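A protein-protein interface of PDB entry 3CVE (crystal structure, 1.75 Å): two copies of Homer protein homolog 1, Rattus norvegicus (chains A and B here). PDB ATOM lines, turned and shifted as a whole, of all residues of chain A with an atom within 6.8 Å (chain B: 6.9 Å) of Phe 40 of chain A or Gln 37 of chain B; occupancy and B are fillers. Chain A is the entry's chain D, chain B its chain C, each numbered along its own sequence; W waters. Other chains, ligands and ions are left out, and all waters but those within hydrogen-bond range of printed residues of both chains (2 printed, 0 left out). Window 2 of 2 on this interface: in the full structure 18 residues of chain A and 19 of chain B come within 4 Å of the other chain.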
ATOM      1  N   SER A  33     -25.127  18.419  13.701  1.00  0.00           N
ATOM      2  CA  SER A  33     -24.181  19.416  14.163  1.00  0.00           C
ATOM      3  C   SER A  33     -24.193  19.515  15.684  1.00  0.00           C
ATOM      4  O   SER A  33     -23.126  19.590  16.306  1.00  0.00           O
ATOM      5  CB  SER A  33     -24.525  20.769  13.519  1.00  0.00           C
ATOM      6  OG  SER A  33     -23.617  21.788  13.882  1.00  0.00           O
ATOM      7  N   GLN A  34     -25.385  19.489  16.286  1.00  0.00           N
ATOM      8  CA  GLN A  34     -25.470  19.567  17.749  1.00  0.00           C
ATOM      9  C   GLN A  34     -24.907  18.261  18.348  1.00  0.00           C
ATOM     10  O   GLN A  34     -24.140  18.307  19.316  1.00  0.00           O
ATOM     11  CB  GLN A  34     -26.892  19.849  18.220  1.00  0.00           C
ATOM     12  CG  GLN A  34     -27.051  20.010  19.727  1.00  0.00           C
ATOM     13  CD  GLN A  34     -26.324  21.212  20.292  1.00  0.00           C
ATOM     14  OE1 GLN A  34     -26.568  22.355  19.884  1.00  0.00           O
ATOM     15  NE2 GLN A  34     -25.415  20.964  21.229  1.00  0.00           N
ATOM     16  N   SER A  35     -25.287  17.125  17.767  1.00  0.00           N
ATOM     17  CA  SER A  35     -24.783  15.813  18.194  1.00  0.00           C
ATOM     18  C   SER A  35     -23.240  15.769  18.224  1.00  0.00           C
ATOM     19  O   SER A  35     -22.627  15.322  19.224  1.00  0.00           O
ATOM     20  CB  SER A  35     -25.340  14.729  17.271  1.00  0.00           C
ATOM     21  OG  SER A  35     -25.284  13.469  17.913  1.00  0.00           O
ATOM     22  N   GLU A  36     -22.626  16.257  17.141  1.00  0.00           N
ATOM     23  CA  GLU A  36     -21.169  16.383  17.017  1.00  0.00           C
ATOM     24  C   GLU A  36     -20.565  17.321  18.070  1.00  0.00           C
ATOM     25  O   GLU A  36     -19.499  17.029  18.634  1.00  0.00           O
ATOM     26  CB  GLU A  36     -20.767  16.894  15.617  1.00  0.00           C
ATOM     27  CG  GLU A  36     -20.919  15.903  14.453  1.00  0.00           C
ATOM     28  CD  GLU A  36     -20.696  16.570  13.105  1.00  0.00           C
ATOM     29  OE1 GLU A  36     -21.120  17.735  12.943  1.00  0.00           O
ATOM     30  OE2 GLU A  36     -20.110  15.928  12.202  1.00  0.00           O
ATOM     31  N   GLN A  37     -21.224  18.462  18.298  1.00  0.00           N
ATOM     32  CA  GLN A  37     -20.749  19.464  19.260  1.00  0.00           C
ATOM     33  C   GLN A  37     -20.806  18.884  20.662  1.00  0.00           C
ATOM     34  O   GLN A  37     -19.880  19.121  21.458  1.00  0.00           O
ATOM     35  CB  GLN A  37     -21.572  20.755  19.185  1.00  0.00           C
ATOM     36  CG  GLN A  37     -21.280  21.535  17.906  1.00  0.00           C
ATOM     37  CD  GLN A  37     -22.177  22.734  17.719  1.00  0.00           C
ATOM     38  OE1 GLN A  37     -22.828  23.204  18.663  1.00  0.00           O
ATOM     39  NE2 GLN A  37     -22.213  23.248  16.487  1.00  0.00           N
ATOM     40  N   ASP A  38     -21.852  18.088  20.935  1.00  0.00           N
ATOM     41  CA  ASP A  38     -21.995  17.445  22.261  1.00  0.00           C
ATOM     42  C   ASP A  38     -20.860  16.466  22.511  1.00  0.00           C
ATOM     43  O   ASP A  38     -20.248  16.462  23.588  1.00  0.00           O
ATOM     44  CB  ASP A  38     -23.357  16.749  22.402  1.00  0.00           C
ATOM     45  CG  ASP A  38     -24.502  17.735  22.471  1.00  0.00           C
ATOM     46  OD1 ASP A  38     -24.219  18.939  22.651  1.00  0.00           O
ATOM     47  OD2 ASP A  38     -25.670  17.314  22.315  1.00  0.00           O
ATOM     48  N   ALA A  39     -20.592  15.634  21.516  1.00  0.00           N
ATOM     49  CA  ALA A  39     -19.535  14.628  21.612  1.00  0.00           C
ATOM     50  C   ALA A  39     -18.141  15.298  21.755  1.00  0.00           C
ATOM     51  O   ALA A  39     -17.300  14.864  22.549  1.00  0.00           O
ATOM     52  CB  ALA A  39     -19.588  13.719  20.425  1.00  0.00           C
ATOM     53  N   PHE A  40     -17.909  16.355  20.980  1.00  0.00           N
ATOM     54  CA  PHE A  40     -16.673  17.168  21.094  1.00  0.00           C
ATOM     55  C   PHE A  40     -16.457  17.637  22.524  1.00  0.00           C
ATOM     56  O   PHE A  40     -15.382  17.443  23.131  1.00  0.00           O
ATOM     57  CB  PHE A  40     -16.831  18.366  20.156  1.00  0.00           C
ATOM     58  CG  PHE A  40     -15.587  19.211  19.997  1.00  0.00           C
ATOM     59  CD1 PHE A  40     -14.590  18.836  19.118  1.00  0.00           C
ATOM     60  CD2 PHE A  40     -15.450  20.393  20.703  1.00  0.00           C
ATOM     61  CE1 PHE A  40     -13.453  19.627  18.940  1.00  0.00           C
ATOM     62  CE2 PHE A  40     -14.301  21.196  20.534  1.00  0.00           C
ATOM     63  CZ  PHE A  40     -13.320  20.807  19.644  1.00  0.00           C
ATOM     64  N   ARG A  41     -17.511  18.227  23.070  1.00  0.00           N
ATOM     65  CA  ARG A  41     -17.522  18.715  24.445  1.00  0.00           C
ATOM     66  C   ARG A  41     -17.247  17.585  25.467  1.00  0.00           C
ATOM     67  O   ARG A  41     -16.476  17.776  26.387  1.00  0.00           O
ATOM     68  CB  ARG A  41     -18.852  19.385  24.728  1.00  0.00           C
ATOM     69  CG  ARG A  41     -19.012  19.955  26.122  1.00  0.00           C
ATOM     70  CD  ARG A  41     -20.235  20.896  26.204  1.00  0.00           C
ATOM     71  NE  ARG A  41     -20.074  22.018  25.275  1.00  0.00           N
ATOM     72  CZ  ARG A  41     -19.432  23.154  25.558  1.00  0.00           C
ATOM     73  NH1 ARG A  41     -18.903  23.349  26.761  1.00  0.00           N
ATOM     74  NH2 ARG A  41     -19.309  24.099  24.633  1.00  0.00           N
ATOM     75  N   SER A  42     -17.846  16.409  25.271  1.00  0.00           N
ATOM     76  CA  SER A  42     -17.564  15.256  26.144  1.00  0.00           C
ATOM     77  C   SER A  42     -16.081  14.831  26.079  1.00  0.00           C
ATOM     78  O   SER A  42     -15.446  14.604  27.122  1.00  0.00           O
ATOM     79  CB  SER A  42     -18.507  14.093  25.814  1.00  0.00           C
ATOM     80  OG  SER A  42     -19.868  14.481  26.128  1.00  0.00           O
ATOM     81  N   ASN A  43     -15.538  14.739  24.872  1.00  0.00           N
ATOM     82  CA  ASN A  43     -14.138  14.381  24.673  1.00  0.00           C
ATOM     83  C   ASN A  43     -13.195  15.412  25.309  1.00  0.00           C
ATOM     84  O   ASN A  43     -12.177  15.063  25.924  1.00  0.00           O
ATOM     85  CB  ASN A  43     -13.812  14.268  23.186  1.00  0.00           C
ATOM     86  CG  ASN A  43     -14.107  12.897  22.615  1.00  0.00           C
ATOM     87  OD1 ASN A  43     -13.301  11.953  22.741  1.00  0.00           O
ATOM     88  ND2 ASN A  43     -15.231  12.779  21.956  1.00  0.00           N
ATOM     89  N   LEU A  44     -13.540  16.681  25.142  1.00  0.00           N
ATOM     90  CA  LEU A  44     -12.730  17.750  25.705  1.00  0.00           C
ATOM     91  C   LEU A  44     -12.758  17.729  27.242  1.00  0.00           C
ATOM     92  O   LEU A  44     -11.730  17.931  27.870  1.00  0.00           O
ATOM     93  CB  LEU A  44     -13.172  19.111  25.165  1.00  0.00           C
ATOM     94  CG  LEU A  44     -12.185  20.246  25.422  1.00  0.00           C
ATOM     95  CD1 LEU A  44     -11.003  20.109  24.440  1.00  0.00           C
ATOM     96  CD2 LEU A  44     -12.936  21.542  25.194  1.00  0.00           C
ATOM     97  N   LYS A  45     -13.925  17.454  27.835  1.00  0.00           N
ATOM     98  CA  LYS A  45     -14.055  17.332  29.298  1.00  0.00           C
ATOM     99  C   LYS A  45     -13.114  16.258  29.881  1.00  0.00           C
ATOM    100  O   LYS A  45     -12.485  16.443  30.938  1.00  0.00           O
ATOM    101  CB  LYS A  45     -15.515  17.053  29.679  1.00  0.00           C
ATOM    102  CG  LYS A  45     -16.380  18.303  29.735  1.00  0.00           C
ATOM    103  CD  LYS A  45     -17.839  17.999  30.155  1.00  0.00           C
ATOM    104  CE  LYS A  45     -17.997  16.726  31.011  1.00  0.00           C
ATOM    105  NZ  LYS A  45     -19.379  16.684  31.612  1.00  0.00           N
ATOM    106  N   GLU B  31     -25.924  28.211  10.733  1.00  0.00           N
ATOM    107  CA  GLU B  31     -24.779  29.098  10.532  1.00  0.00           C
ATOM    108  C   GLU B  31     -24.264  29.661  11.858  1.00  0.00           C
ATOM    109  O   GLU B  31     -23.053  29.660  12.116  1.00  0.00           O
ATOM    110  CB  GLU B  31     -25.169  30.229   9.578  1.00  0.00           C
ATOM    111  CG  GLU B  31     -25.618  29.733   8.200  1.00  0.00           C
ATOM    112  CD  GLU B  31     -25.813  30.846   7.182  1.00  0.00           C
ATOM    113  OE1 GLU B  31     -26.234  31.970   7.566  1.00  0.00           O
ATOM    114  OE2 GLU B  31     -25.547  30.594   5.978  1.00  0.00           O
ATOM    115  N   LYS B  32     -25.190  30.107  12.708  1.00  0.00           N
ATOM    116  CA  LYS B  32     -24.845  30.610  14.046  1.00  0.00           C
ATOM    117  C   LYS B  32     -24.132  29.532  14.857  1.00  0.00           C
ATOM    118  O   LYS B  32     -23.077  29.780  15.464  1.00  0.00           O
ATOM    119  CB  LYS B  32     -26.100  31.090  14.788  1.00  0.00           C
ATOM    120  CG  LYS B  32     -25.836  31.672  16.191  1.00  0.00           C
ATOM    121  CD  LYS B  32     -27.133  32.147  16.852  1.00  0.00           C
ATOM    122  CE  LYS B  32     -27.844  33.216  16.013  1.00  0.00           C
ATOM    123  NZ  LYS B  32     -27.111  34.521  16.070  1.00  0.00           N
ATOM    124  N   SER B  33     -24.711  28.333  14.848  1.00  0.00           N
ATOM    125  CA  SER B  33     -24.142  27.206  15.586  1.00  0.00           C
ATOM    126  C   SER B  33     -22.730  26.909  15.075  1.00  0.00           C
ATOM    127  O   SER B  33     -21.796  26.728  15.868  1.00  0.00           O
ATOM    128  CB  SER B  33     -25.034  25.968  15.451  1.00  0.00           C
ATOM    129  OG  SER B  33     -24.506  24.878  16.197  1.00  0.00           O
ATOM    130  N   GLN B  34     -22.577  26.872  13.753  1.00  0.00           N
ATOM    131  CA  GLN B  34     -21.305  26.472  13.144  1.00  0.00           C
ATOM    132  C   GLN B  34     -20.213  27.527  13.361  1.00  0.00           C
ATOM    133  O   GLN B  34     -19.034  27.178  13.517  1.00  0.00           O
ATOM    134  CB  GLN B  34     -21.475  26.084  11.669  1.00  0.00           C
ATOM    135  CG  GLN B  34     -22.365  24.820  11.465  1.00  0.00           C
ATOM    136  CD  GLN B  34     -22.380  24.258  10.035  1.00  0.00           C
ATOM    137  OE1 GLN B  34     -22.041  24.944   9.066  1.00  0.00           O
ATOM    138  NE2 GLN B  34     -22.791  22.996   9.908  1.00  0.00           N
ATOM    139  N   SER B  35     -20.627  28.797  13.408  1.00  0.00           N
ATOM    140  CA  SER B  35     -19.747  29.940  13.664  1.00  0.00           C
ATOM    141  C   SER B  35     -19.196  29.881  15.084  1.00  0.00           C
ATOM    142  O   SER B  35     -17.985  30.013  15.293  1.00  0.00           O
ATOM    143  CB  SER B  35     -20.506  31.253  13.471  1.00  0.00           C
ATOM    144  OG  SER B  35     -20.755  31.493  12.098  1.00  0.00           O
ATOM    145  N   GLU B  36     -20.104  29.682  16.039  1.00  0.00           N
ATOM    146  CA  GLU B  36     -19.773  29.478  17.449  1.00  0.00           C
ATOM    147  C   GLU B  36     -18.794  28.315  17.639  1.00  0.00           C
ATOM    148  O   GLU B  36     -17.814  28.435  18.387  1.00  0.00           O
ATOM    149  CB  GLU B  36     -21.046  29.254  18.273  1.00  0.00           C
ATOM    150  CG  GLU B  36     -21.938  30.505  18.363  1.00  0.00           C
ATOM    151  CD  GLU B  36     -23.304  30.254  18.982  1.00  0.00           C
ATOM    152  OE1 GLU B  36     -23.645  29.089  19.285  1.00  0.00           O
ATOM    153  OE2 GLU B  36     -24.052  31.242  19.162  1.00  0.00           O
ATOM    154  N   GLN B  37     -19.042  27.200  16.956  1.00  0.00           N
ATOM    155  CA  GLN B  37     -18.167  26.052  17.115  1.00  0.00           C
ATOM    156  C   GLN B  37     -16.769  26.383  16.559  1.00  0.00           C
ATOM    157  O   GLN B  37     -15.780  26.007  17.162  1.00  0.00           O
ATOM    158  CB  GLN B  37     -18.770  24.781  16.485  1.00  0.00           C
ATOM    159  CG  GLN B  37     -17.909  23.496  16.598  1.00  0.00           C
ATOM    160  CD  GLN B  37     -17.465  23.091  18.019  1.00  0.00           C
ATOM    161  OE1 GLN B  37     -16.306  22.691  18.218  1.00  0.00           O
ATOM    162  NE2 GLN B  37     -18.369  23.167  18.987  1.00  0.00           N
ATOM    163  N   ASP B  38     -16.713  27.116  15.437  1.00  0.00           N
ATOM    164  CA  ASP B  38     -15.458  27.529  14.779  1.00  0.00           C
ATOM    165  C   ASP B  38     -14.610  28.382  15.707  1.00  0.00           C
ATOM    166  O   ASP B  38     -13.371  28.269  15.728  1.00  0.00           O
ATOM    167  CB  ASP B  38     -15.753  28.420  13.554  1.00  0.00           C
ATOM    168  CG  ASP B  38     -16.224  27.660  12.331  1.00  0.00           C
ATOM    169  OD1 ASP B  38     -16.196  26.408  12.277  1.00  0.00           O
ATOM    170  OD2 ASP B  38     -16.632  28.364  11.379  1.00  0.00           O
ATOM    171  N   ALA B  39     -15.291  29.272  16.435  1.00  0.00           N
ATOM    172  CA  ALA B  39     -14.646  30.196  17.361  1.00  0.00           C
ATOM    173  C   ALA B  39     -14.132  29.409  18.559  1.00  0.00           C
ATOM    174  O   ALA B  39     -13.051  29.672  19.063  1.00  0.00           O
ATOM    175  CB  ALA B  39     -15.616  31.254  17.817  1.00  0.00           C
ATOM    176  N   PHE B  40     -14.938  28.445  18.996  1.00  0.00           N
ATOM    177  CA  PHE B  40     -14.560  27.502  20.057  1.00  0.00           C
ATOM    178  C   PHE B  40     -13.292  26.749  19.621  1.00  0.00           C
ATOM    179  O   PHE B  40     -12.311  26.740  20.367  1.00  0.00           O
ATOM    180  CB  PHE B  40     -15.754  26.561  20.328  1.00  0.00           C
ATOM    181  CG  PHE B  40     -15.620  25.691  21.567  1.00  0.00           C
ATOM    182  CD1 PHE B  40     -15.207  26.221  22.783  1.00  0.00           C
ATOM    183  CD2 PHE B  40     -15.969  24.351  21.516  1.00  0.00           C
ATOM    184  CE1 PHE B  40     -15.111  25.410  23.926  1.00  0.00           C
ATOM    185  CE2 PHE B  40     -15.882  23.543  22.643  1.00  0.00           C
ATOM    186  CZ  PHE B  40     -15.457  24.078  23.852  1.00  0.00           C
ATOM    187  N   ARG B  41     -13.290  26.178  18.410  1.00  0.00           N
ATOM    188  CA  ARG B  41     -12.144  25.401  17.911  1.00  0.00           C
ATOM    189  C   ARG B  41     -10.868  26.249  17.824  1.00  0.00           C
ATOM    190  O   ARG B  41      -9.808  25.818  18.273  1.00  0.00           O
ATOM    191  CB  ARG B  41     -12.414  24.742  16.551  1.00  0.00           C
ATOM    192  CG  ARG B  41     -13.507  23.661  16.545  1.00  0.00           C
ATOM    193  CD  ARG B  41     -13.485  22.872  15.234  1.00  0.00           C
ATOM    194  NE  ARG B  41     -14.773  22.240  14.914  1.00  0.00           N
ATOM    195  CZ  ARG B  41     -15.715  22.811  14.163  1.00  0.00           C
ATOM    196  NH1 ARG B  41     -15.537  24.037  13.680  1.00  0.00           N
ATOM    197  NH2 ARG B  41     -16.846  22.163  13.907  1.00  0.00           N
ATOM    198  N   SER B  42     -10.972  27.447  17.250  1.00  0.00           N
ATOM    199  CA  SER B  42      -9.813  28.367  17.204  1.00  0.00           C
ATOM    200  C   SER B  42      -9.221  28.702  18.592  1.00  0.00           C
ATOM    201  O   SER B  42      -7.981  28.773  18.771  1.00  0.00           O
ATOM    202  CB  SER B  42     -10.155  29.648  16.421  1.00  0.00           C
ATOM    203  OG  SER B  42     -10.897  30.555  17.219  1.00  0.00           O
ATOM    204  N   ASN B  43     -10.082  28.904  19.581  1.00  0.00           N
ATOM    205  CA  ASN B  43      -9.590  29.258  20.907  1.00  0.00           C
ATOM    206  C   ASN B  43      -8.867  28.074  21.557  1.00  0.00           C
ATOM    207  O   ASN B  43      -7.892  28.243  22.310  1.00  0.00           O
ATOM    208  CB  ASN B  43     -10.715  29.739  21.809  1.00  0.00           C
ATOM    209  CG  ASN B  43     -11.098  31.196  21.572  1.00  0.00           C
ATOM    210  OD1 ASN B  43     -10.250  32.048  21.292  1.00  0.00           O
ATOM    211  ND2 ASN B  43     -12.387  31.490  21.729  1.00  0.00           N
ATOM    212  N   LEU B  44      -9.343  26.870  21.253  1.00  0.00           N
ATOM    213  CA  LEU B  44      -8.682  25.662  21.754  1.00  0.00           C
ATOM    214  C   LEU B  44      -7.350  25.405  21.037  1.00  0.00           C
ATOM    215  O   LEU B  44      -6.402  24.866  21.640  1.00  0.00           O
ATOM    216  CB  LEU B  44      -9.606  24.459  21.622  1.00  0.00           C
ATOM    217  CG  LEU B  44     -10.819  24.518  22.554  1.00  0.00           C
ATOM    218  CD1 LEU B  44     -11.903  23.570  22.066  1.00  0.00           C
ATOM    219  CD2 LEU B  44     -10.439  24.184  23.996  1.00  0.00           C
HETATM  220  O   HOH W   1     -19.046  21.706  21.926  1.00  0.00           O
HETATM  221  O   HOH W   2     -26.587  23.466  16.898  1.00  0.00           O
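Among the printed residues, pairs that only touch across the chains: Phe 40 of chain A with Gln 37 of chain B, Gln 37 of chain A with Gln 37 of chain B, Phe 40 of chain A with Phe 40 of chain B, Phe 40 of chain A with Leu 44 of chain B, Leu 44 of chain A with Phe 40 of chain B, Leu 44 of chain A with Leu 44 of chain B, Arg 41 of chain A with Phe 40 of chain B and Ser 33 of chain A with Ser 33 of chain B.
Of chain B, only Gln 37 (3.4 Å), Phe 40 (3.5 Å) and Leu 44 (3.7 Å) come within 4 Å of Phe 40 of chain A. Of chain A, only Gln 37 (3.5 Å) and Phe 40 (3.4 Å) come within 4 Å of Gln 37 of chain B. Of the printed residues of chain B, Leu 44 of chain A touches Phe 40 and Leu 44. Of the printed residues of chain A, Leu 44 of chain B touches Phe 40 (3.7 Å) and Leu 44 (3.8 Å). Glu 36 of chain B touches none of the printed residues of chain A. Ser 35 of chain B touches none of the printed residues of chain A.
Ser 33 of chain B touches its own counterpart, Ser 33 of chain A. Phe 40 of chain A touches Leu 44 of chain B, and with the chains exchanged Leu 44 of chain A touches Phe 40 of chain B. Arg 41 of chain A touches Phe 40 of chain B, but with the chains exchanged Phe 40 of chain A does not touch Arg 41 of chain B (4.2 Å). Leu 44 of chain A touches its own counterpart, Leu 44 of chain B. Positions printed for both chains: 33, 34, 35, 36, 37, 38, 39, 40, 41, 42, 43 and 44.
Of the 14 printed residues of chain B, 4 touch a printed residue of chain A. Printed residues of chain B that touch a printed residue of chain A: Ser 33, Gln 37, Phe 40 and Leu 44. Among the printed residues, 9 pairs touch across the chains. Among the printed residues, no Asp or Glu carboxylate lies within 4 Å of a Lys or Arg side-chain nitrogen of the other chain.
Water W2 lies within hydrogen-bond range of the side-chain hydroxyl (OG) of Ser 33 of chain B (2.6 Å) and the side-chain amide oxygen (OE1) of Gln 34 of chain A (3.2 Å). Water W1 lies within hydrogen-bond range of O of Gln 37 of chain A (2.8 Å) and NE2 of Gln 37 of chain B (3.4 Å).
OG of Ser 33 of chain A is in hydrogen-bond range of NE2 of Gln 37 of chain A (3.3 Å).
OG of Ser 33 of chain B is in hydrogen-bond range of NE2 of Gln 37 of chain A (2.8 Å).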
